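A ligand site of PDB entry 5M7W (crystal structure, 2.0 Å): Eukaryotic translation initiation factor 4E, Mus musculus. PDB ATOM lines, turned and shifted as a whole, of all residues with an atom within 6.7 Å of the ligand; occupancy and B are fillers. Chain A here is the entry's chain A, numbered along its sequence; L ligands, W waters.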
ATOM      1  N   PHE A  21      -3.566 -14.516  -9.868  1.00  0.00           N
ATOM      2  CA  PHE A  21      -4.284 -15.480  -9.049  1.00  0.00           C
ATOM      3  C   PHE A  21      -4.007 -15.104  -7.607  1.00  0.00           C
ATOM      4  O   PHE A  21      -2.848 -14.877  -7.233  1.00  0.00           O
ATOM      5  CB  PHE A  21      -3.817 -16.921  -9.315  1.00  0.00           C
ATOM      6  CG  PHE A  21      -4.351 -17.943  -8.319  1.00  0.00           C
ATOM      7  CD1 PHE A  21      -3.694 -18.169  -7.104  1.00  0.00           C
ATOM      8  CD2 PHE A  21      -5.500 -18.677  -8.594  1.00  0.00           C
ATOM      9  CE1 PHE A  21      -4.179 -19.082  -6.189  1.00  0.00           C
ATOM     10  CE2 PHE A  21      -5.990 -19.612  -7.677  1.00  0.00           C
ATOM     11  CZ  PHE A  21      -5.330 -19.806  -6.462  1.00  0.00           C
ATOM     12  N   ASN A  23      -4.815 -16.623  -3.789  1.00  0.00           N
ATOM     13  CA  ASN A  23      -5.392 -17.688  -2.992  1.00  0.00           C
ATOM     14  C   ASN A  23      -6.458 -17.110  -2.077  1.00  0.00           C
ATOM     15  O   ASN A  23      -6.183 -16.277  -1.202  1.00  0.00           O
ATOM     16  CB  ASN A  23      -4.292 -18.386  -2.174  1.00  0.00           C
ATOM     17  CG  ASN A  23      -4.762 -19.696  -1.600  1.00  0.00           C
ATOM     18  OD1 ASN A  23      -5.599 -20.391  -2.204  1.00  0.00           O
ATOM     19  ND2 ASN A  23      -4.233 -20.055  -0.433  1.00  0.00           N
ATOM     20  N   TRP A  29     -10.885 -22.534  -7.184  1.00  0.00           N
ATOM     21  CA  TRP A  29      -9.582 -22.183  -7.746  1.00  0.00           C
ATOM     22  C   TRP A  29      -9.745 -21.351  -9.010  1.00  0.00           C
ATOM     23  O   TRP A  29      -9.062 -20.336  -9.182  1.00  0.00           O
ATOM     24  CB  TRP A  29      -8.792 -23.460  -8.069  1.00  0.00           C
ATOM     25  CG  TRP A  29      -7.468 -23.164  -8.647  1.00  0.00           C
ATOM     26  CD1 TRP A  29      -6.309 -22.918  -7.954  1.00  0.00           C
ATOM     27  CD2 TRP A  29      -7.156 -23.043 -10.016  1.00  0.00           C
ATOM     28  NE1 TRP A  29      -5.282 -22.667  -8.835  1.00  0.00           N
ATOM     29  CE2 TRP A  29      -5.777 -22.748 -10.111  1.00  0.00           C
ATOM     30  CE3 TRP A  29      -7.896 -23.168 -11.180  1.00  0.00           C
ATOM     31  CZ2 TRP A  29      -5.137 -22.554 -11.334  1.00  0.00           C
ATOM     32  CZ3 TRP A  29      -7.249 -22.984 -12.397  1.00  0.00           C
ATOM     33  CH2 TRP A  29      -5.889 -22.679 -12.456  1.00  0.00           C
ATOM     34  N   GLN A  30     -10.656 -21.773  -9.914  1.00  0.00           N
ATOM     35  CA  GLN A  30     -10.870 -21.040 -11.154  1.00  0.00           C
ATOM     36  C   GLN A  30     -11.400 -19.629 -10.909  1.00  0.00           C
ATOM     37  O   GLN A  30     -11.042 -18.692 -11.617  1.00  0.00           O
ATOM     38  CB  GLN A  30     -11.815 -21.807 -12.085  1.00  0.00           C
ATOM     39  N   LEU A  33      -8.735 -17.000 -10.352  1.00  0.00           N
ATOM     40  CA  LEU A  33      -7.930 -16.647 -11.513  1.00  0.00           C
ATOM     41  C   LEU A  33      -8.578 -15.499 -12.272  1.00  0.00           C
ATOM     42  O   LEU A  33      -9.712 -15.639 -12.739  1.00  0.00           O
ATOM     43  CB  LEU A  33      -7.815 -17.870 -12.418  1.00  0.00           C
ATOM     44  CG  LEU A  33      -6.890 -17.879 -13.619  1.00  0.00           C
ATOM     45  CD1 LEU A  33      -5.446 -17.559 -13.200  1.00  0.00           C
ATOM     46  CD2 LEU A  33      -7.013 -19.275 -14.226  1.00  0.00           C
ATOM     47  N   GLY A  61       0.793 -17.316  -1.852  1.00  0.00           N
ATOM     48  CA  GLY A  61      -0.445 -17.827  -2.398  1.00  0.00           C
ATOM     49  C   GLY A  61      -0.880 -17.169  -3.708  1.00  0.00           C
ATOM     50  O   GLY A  61      -1.899 -17.577  -4.275  1.00  0.00           O
ATOM     51  N   ASP A  63      -0.210 -15.878  -7.787  1.00  0.00           N
ATOM     52  CA  ASP A  63       0.539 -16.205  -8.995  1.00  0.00           C
ATOM     53  C   ASP A  63       0.414 -15.072 -10.003  1.00  0.00           C
ATOM     54  O   ASP A  63      -0.566 -14.312 -10.010  1.00  0.00           O
ATOM     55  CB  ASP A  63       0.055 -17.502  -9.750  1.00  0.00           C
ATOM     56  CG  ASP A  63      -0.324 -18.640  -8.844  1.00  0.00           C
ATOM     57  OD1 ASP A  63       0.311 -18.829  -7.790  1.00  0.00           O
ATOM     58  OD2 ASP A  63      -1.215 -19.416  -9.257  1.00  0.00           O
ATOM     59  N   PRO A  73      -4.510 -19.809 -18.458  1.00  0.00           N
ATOM     60  CA  PRO A  73      -3.418 -20.479 -17.739  1.00  0.00           C
ATOM     61  C   PRO A  73      -3.932 -21.644 -16.893  1.00  0.00           C
ATOM     62  O   PRO A  73      -3.724 -21.694 -15.686  1.00  0.00           O
ATOM     63  CB  PRO A  73      -2.828 -19.343 -16.895  1.00  0.00           C
ATOM     64  CG  PRO A  73      -3.946 -18.400 -16.664  1.00  0.00           C
ATOM     65  CD  PRO A  73      -5.009 -18.636 -17.720  1.00  0.00           C
ATOM     66  N   MET A  74      -4.640 -22.575 -17.534  1.00  0.00           N
ATOM     67  CA  MET A  74      -5.160 -23.727 -16.813  1.00  0.00           C
ATOM     68  C   MET A  74      -5.009 -24.989 -17.637  1.00  0.00           C
ATOM     69  O   MET A  74      -5.044 -24.959 -18.870  1.00  0.00           O
ATOM     70  CB  MET A  74      -6.639 -23.517 -16.376  1.00  0.00           C
ATOM     71  CG  MET A  74      -7.556 -23.026 -17.472  1.00  0.00           C
ATOM     72  SD  MET A  74      -9.309 -23.078 -17.014  1.00  0.00           S
ATOM     73  CE  MET A  74      -9.396 -21.949 -15.663  1.00  0.00           C
ATOM     74  N   TRP A  75      -4.825 -26.111 -16.934  1.00  0.00           N
ATOM     75  CA  TRP A  75      -4.655 -27.414 -17.585  1.00  0.00           C
ATOM     76  C   TRP A  75      -5.751 -27.697 -18.601  1.00  0.00           C
ATOM     77  O   TRP A  75      -5.498 -28.358 -19.611  1.00  0.00           O
ATOM     78  CB  TRP A  75      -4.645 -28.556 -16.553  1.00  0.00           C
ATOM     79  CG  TRP A  75      -3.672 -28.367 -15.409  1.00  0.00           C
ATOM     80  CD1 TRP A  75      -2.401 -27.831 -15.469  1.00  0.00           C
ATOM     81  CD2 TRP A  75      -3.868 -28.784 -14.050  1.00  0.00           C
ATOM     82  NE1 TRP A  75      -1.824 -27.853 -14.215  1.00  0.00           N
ATOM     83  CE2 TRP A  75      -2.692 -28.444 -13.337  1.00  0.00           C
ATOM     84  CE3 TRP A  75      -4.915 -29.405 -13.370  1.00  0.00           C
ATOM     85  CZ2 TRP A  75      -2.555 -28.693 -11.994  1.00  0.00           C
ATOM     86  CZ3 TRP A  75      -4.777 -29.654 -12.027  1.00  0.00           C
ATOM     87  CH2 TRP A  75      -3.594 -29.295 -11.352  1.00  0.00           C
ATOM     88  N   GLU A  76      -6.972 -27.243 -18.328  1.00  0.00           N
ATOM     89  CA  GLU A  76      -8.098 -27.688 -19.138  1.00  0.00           C
ATOM     90  C   GLU A  76      -8.185 -26.970 -20.480  1.00  0.00           C
ATOM     91  O   GLU A  76      -9.005 -27.368 -21.297  1.00  0.00           O
ATOM     92  CB  GLU A  76      -9.435 -27.553 -18.381  1.00  0.00           C
ATOM     93  CG  GLU A  76      -9.513 -28.435 -17.126  1.00  0.00           C
ATOM     94  CD  GLU A  76      -8.922 -27.808 -15.871  1.00  0.00           C
ATOM     95  OE1 GLU A  76      -9.304 -28.257 -14.764  1.00  0.00           O
ATOM     96  OE2 GLU A  76      -8.025 -26.949 -15.973  1.00  0.00           O
ATOM     97  N   ARG A  85       4.979 -28.786 -18.297  1.00  0.00           N
ATOM     98  CA  ARG A  85       5.695 -27.597 -17.844  1.00  0.00           C
ATOM     99  C   ARG A  85       7.137 -27.931 -17.492  1.00  0.00           C
ATOM    100  O   ARG A  85       7.413 -28.956 -16.862  1.00  0.00           O
ATOM    101  CB  ARG A  85       5.007 -26.931 -16.650  1.00  0.00           C
ATOM    102  CG  ARG A  85       5.056 -27.734 -15.338  1.00  0.00           C
ATOM    103  CD  ARG A  85       4.356 -27.009 -14.191  1.00  0.00           C
ATOM    104  NE  ARG A  85       4.432 -27.784 -12.940  1.00  0.00           N
ATOM    105  CZ  ARG A  85       3.920 -27.377 -11.777  1.00  0.00           C
ATOM    106  NH1 ARG A  85       3.311 -26.204 -11.677  1.00  0.00           N
ATOM    107  NH2 ARG A  85       4.063 -28.145 -10.696  1.00  0.00           N
ATOM    108  N   VAL A 126       4.256 -19.380 -15.711  1.00  0.00           N
ATOM    109  CA  VAL A 126       3.586 -19.184 -14.442  1.00  0.00           C
ATOM    110  C   VAL A 126       4.657 -19.062 -13.375  1.00  0.00           C
ATOM    111  O   VAL A 126       5.587 -19.880 -13.342  1.00  0.00           O
ATOM    112  CB  VAL A 126       2.653 -20.371 -14.094  1.00  0.00           C
ATOM    113  CG1 VAL A 126       2.057 -20.186 -12.684  1.00  0.00           C
ATOM    114  CG2 VAL A 126       1.566 -20.561 -15.145  1.00  0.00           C
ATOM    115  N   ASN A 128       4.594 -19.157  -9.210  1.00  0.00           N
ATOM    116  CA  ASN A 128       3.857 -19.323  -7.972  1.00  0.00           C
ATOM    117  C   ASN A 128       4.695 -18.779  -6.815  1.00  0.00           C
ATOM    118  O   ASN A 128       5.836 -19.222  -6.604  1.00  0.00           O
ATOM    119  CB  ASN A 128       3.490 -20.780  -7.695  1.00  0.00           C
ATOM    120  CG  ASN A 128       2.840 -21.480  -8.907  1.00  0.00           C
ATOM    121  OD1 ASN A 128       1.658 -21.280  -9.203  1.00  0.00           O
ATOM    122  ND2 ASN A 128       3.577 -22.397  -9.526  1.00  0.00           N
ATOM    123  N   ARG A 130       4.988 -18.859  -3.020  1.00  0.00           N
ATOM    124  CA  ARG A 130       4.530 -19.733  -1.954  1.00  0.00           C
ATOM    125  C   ARG A 130       5.500 -19.706  -0.784  1.00  0.00           C
ATOM    126  O   ARG A 130       6.711 -19.620  -0.955  1.00  0.00           O
ATOM    127  CB  ARG A 130       4.399 -21.198  -2.431  1.00  0.00           C
ATOM    128  CG  ARG A 130       3.545 -21.386  -3.660  1.00  0.00           C
ATOM    129  CD  ARG A 130       2.084 -21.211  -3.295  1.00  0.00           C
ATOM    130  NE  ARG A 130       1.220 -21.605  -4.390  1.00  0.00           N
ATOM    131  CZ  ARG A 130       0.710 -20.748  -5.264  1.00  0.00           C
ATOM    132  NH1 ARG A 130       1.007 -19.442  -5.169  1.00  0.00           N
ATOM    133  NH2 ARG A 130      -0.067 -21.176  -6.251  1.00  0.00           N
ATOM    134  N   ALA A 131       4.916 -19.830   0.410  1.00  0.00           N
ATOM    135  CA  ALA A 131       5.729 -19.826   1.627  1.00  0.00           C
ATOM    136  C   ALA A 131       6.692 -20.997   1.639  1.00  0.00           C
ATOM    137  O   ALA A 131       7.832 -20.885   2.101  1.00  0.00           O
ATOM    138  CB  ALA A 131       4.837 -19.858   2.863  1.00  0.00           C
ATOM    139  N   LYS A 132       6.241 -22.151   1.144  1.00  0.00           N
ATOM    140  CA  LYS A 132       7.063 -23.358   1.181  1.00  0.00           C
ATOM    141  C   LYS A 132       8.176 -23.340   0.150  1.00  0.00           C
ATOM    142  O   LYS A 132       9.055 -24.211   0.187  1.00  0.00           O
ATOM    143  CB  LYS A 132       6.184 -24.600   0.976  1.00  0.00           C
ATOM    144  N   GLY A 133       8.183 -22.364  -0.763  1.00  0.00           N
ATOM    145  CA  GLY A 133       9.161 -22.327  -1.828  1.00  0.00           C
ATOM    146  C   GLY A 133       8.497 -21.889  -3.118  1.00  0.00           C
ATOM    147  O   GLY A 133       7.433 -22.411  -3.477  1.00  0.00           O
ATOM    148  N   LYS A 135       7.899 -21.186  -7.284  1.00  0.00           N
ATOM    149  CA  LYS A 135       8.055 -21.939  -8.510  1.00  0.00           C
ATOM    150  C   LYS A 135       7.932 -21.007  -9.710  1.00  0.00           C
ATOM    151  O   LYS A 135       7.129 -20.076  -9.707  1.00  0.00           O
ATOM    152  CB  LYS A 135       6.984 -23.047  -8.659  1.00  0.00           C
ATOM    153  CG  LYS A 135       6.775 -23.934  -7.464  1.00  0.00           C
ATOM    154  CD  LYS A 135       6.182 -25.248  -7.943  1.00  0.00           C
ATOM    155  CE  LYS A 135       6.052 -26.260  -6.828  1.00  0.00           C
ATOM    156  NZ  LYS A 135       4.590 -26.523  -6.610  1.00  0.00           N
ATOM    157  N   TRP A 139       5.041 -23.335 -19.748  1.00  0.00           N
ATOM    158  CA  TRP A 139       4.052 -24.313 -20.196  1.00  0.00           C
ATOM    159  C   TRP A 139       4.111 -24.487 -21.712  1.00  0.00           C
ATOM    160  O   TRP A 139       4.071 -23.504 -22.454  1.00  0.00           O
ATOM    161  CB  TRP A 139       2.644 -23.900 -19.812  1.00  0.00           C
ATOM    162  CG  TRP A 139       2.290 -23.983 -18.369  1.00  0.00           C
ATOM    163  CD1 TRP A 139       3.142 -23.888 -17.298  1.00  0.00           C
ATOM    164  CD2 TRP A 139       0.980 -24.205 -17.829  1.00  0.00           C
ATOM    165  NE1 TRP A 139       2.430 -24.016 -16.120  1.00  0.00           N
ATOM    166  CE2 TRP A 139       1.105 -24.221 -16.415  1.00  0.00           C
ATOM    167  CE3 TRP A 139      -0.298 -24.387 -18.399  1.00  0.00           C
ATOM    168  CZ2 TRP A 139      -0.005 -24.421 -15.563  1.00  0.00           C
ATOM    169  CZ3 TRP A 139      -1.399 -24.584 -17.551  1.00  0.00           C
ATOM    170  CH2 TRP A 139      -1.233 -24.599 -16.151  1.00  0.00           C
ATOM    171  N   THR A 176       0.383 -34.078 -13.182  1.00  0.00           N
ATOM    172  CA  THR A 176       0.195 -33.102 -12.109  1.00  0.00           C
ATOM    173  C   THR A 176      -1.245 -33.071 -11.625  1.00  0.00           C
ATOM    174  O   THR A 176      -1.501 -32.992 -10.418  1.00  0.00           O
ATOM    175  CB  THR A 176       0.616 -31.716 -12.600  1.00  0.00           C
ATOM    176  OG1 THR A 176       1.854 -31.807 -13.317  1.00  0.00           O
ATOM    177  CG2 THR A 176       0.786 -30.754 -11.441  1.00  0.00           C
HETATM  178  C1  LIG L   1      -7.581 -26.773 -12.147  1.00  0.00           C
HETATM  179  C2  LIG L   1      -3.887 -25.553 -10.002  1.00  0.00           C
HETATM  180  C3  LIG L   1      -5.802 -26.217 -10.719  1.00  0.00           C
HETATM  181  C4  LIG L   1      -5.035 -25.845 -11.809  1.00  0.00           C
HETATM  182  C5  LIG L   1      -5.575 -25.932 -13.105  1.00  0.00           C
HETATM  183  O1  LIG L   1      -0.937 -24.003  -6.393  1.00  0.00           O
HETATM  184  P1  LIG L   1      -0.627 -25.248  -7.184  1.00  0.00           P
HETATM  185  O2  LIG L   1      -0.055 -24.975  -8.560  1.00  0.00           O
HETATM  186  O3  LIG L   1       0.409 -26.240  -6.477  1.00  0.00           O
HETATM  187  P2  LIG L   1       1.278 -25.784  -5.215  1.00  0.00           P
HETATM  188  O4  LIG L   1       1.902 -27.001  -4.659  1.00  0.00           O
HETATM  189  S1  LIG L   1       2.572 -24.490  -5.813  1.00  0.00           S
HETATM  190  O5  LIG L   1       0.214 -25.080  -4.247  1.00  0.00           O
HETATM  191  P3  LIG L   1       0.332 -25.100  -2.664  1.00  0.00           P
HETATM  192  O6  LIG L   1      -0.745 -24.022  -2.121  1.00  0.00           O
HETATM  193  O7  LIG L   1      -0.001 -26.495  -2.192  1.00  0.00           O
HETATM  194  O8  LIG L   1       1.728 -24.693  -2.258  1.00  0.00           O
HETATM  195  O9  LIG L   1      -2.042 -25.995  -7.262  1.00  0.00           O
HETATM  196  C6  LIG L   1      -2.773 -26.113  -6.048  1.00  0.00           C
HETATM  197  C7  LIG L   1      -4.140 -26.642  -6.434  1.00  0.00           C
HETATM  198  C8  LIG L   1      -4.040 -27.844  -7.353  1.00  0.00           C
HETATM  199  O10 LIG L   1      -3.892 -29.063  -6.622  1.00  0.00           O
HETATM  200  C9  LIG L   1      -5.374 -27.820  -8.026  1.00  0.00           C
HETATM  201  O11 LIG L   1      -6.297 -28.333  -7.074  1.00  0.00           O
HETATM  202  C10 LIG L   1      -7.670 -28.106  -7.393  1.00  0.00           C
HETATM  203  C11 LIG L   1      -5.580 -26.338  -8.257  1.00  0.00           C
HETATM  204  O12 LIG L   1      -4.858 -25.673  -7.209  1.00  0.00           O
HETATM  205  N1  LIG L   1      -5.089 -26.032  -9.628  1.00  0.00           N
HETATM  206  N2  LIG L   1      -7.063 -26.680 -10.908  1.00  0.00           N
HETATM  207  N3  LIG L   1      -8.843 -27.237 -12.276  1.00  0.00           N
HETATM  208  N4  LIG L   1      -6.843 -26.409 -13.231  1.00  0.00           N
HETATM  209  O13 LIG L   1      -4.911 -25.589 -14.263  1.00  0.00           O
HETATM  210  N5  LIG L   1      -3.834 -25.431 -11.341  1.00  0.00           N
HETATM  211  C12 LIG L   1      -2.636 -24.922 -12.074  1.00  0.00           C
HETATM  212  O   HOH W   1       2.444 -24.900  -9.379  1.00  0.00           O
HETATM  213  O   HOH W   2      -0.756 -22.106 -11.576  1.00  0.00           O
HETATM  214  O   HOH W   3       0.524 -29.254  -5.872  1.00  0.00           O
HETATM  215  O   HOH W   4       0.143 -27.341  -9.806  1.00  0.00           O
HETATM  216  O   HOH W   5      -3.104 -22.255  -6.052  1.00  0.00           O
HETATM  217  O   HOH W   6      -2.620 -21.837  -8.562  1.00  0.00           O
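An oxygen (O13) of the ligand is in hydrogen-bond range of the backbone NH (N) of Trp 75 (2.7 Å).
OE1 of Glu 76 is in hydrogen-bond range of N3 of the ligand.
The guanidinium group (NH2) of Arg 130 is in salt-bridge range of an oxygen (O1) of the ligand, at 3.0 Å.
The side-chain amino group (NZ) of Lys 135 lies close to a sulfur (S1) of the ligand (3.0 Å).
The indole nitrogen (NE1) of Trp 29 lies close to an oxygen (O12) of the ligand, at 3.4 Å.
NH2 of Arg 130 is in hydrogen-bond range of OD1 of Asn 128, at 3.4 Å.
The guanidinium group (NH1) of Arg 130 is in salt-bridge range of the side-chain carboxylate (OD1) of Asp 63, 2.8 Å away.
The backbone carbonyl oxygen of Lys 135 lies within hydrogen-bond range of the backbone NH of Asn 128 (2.7 Å).
Merely in contact with the ligand: Met 74 (3.2 Å).
Of the 21 residues printed, 6 come within 4 Å of the ligand.
The nearest printed residue that does not touch the ligand is Asn 128 (4.1 Å).
Water W1 lies within hydrogen-bond range of O2 of the ligand, ND2 of Asn 128 and NH1 of Arg 85.
Water W5 bridges an oxygen (O1) of the ligand and the guanidinium group of Arg 130.
Water W6 lies within hydrogen-bond range of NE1 of Trp 29 (2.8 Å), OD2 of Asp 63 (2.9 Å) and O1 of the ligand (3.5 Å).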
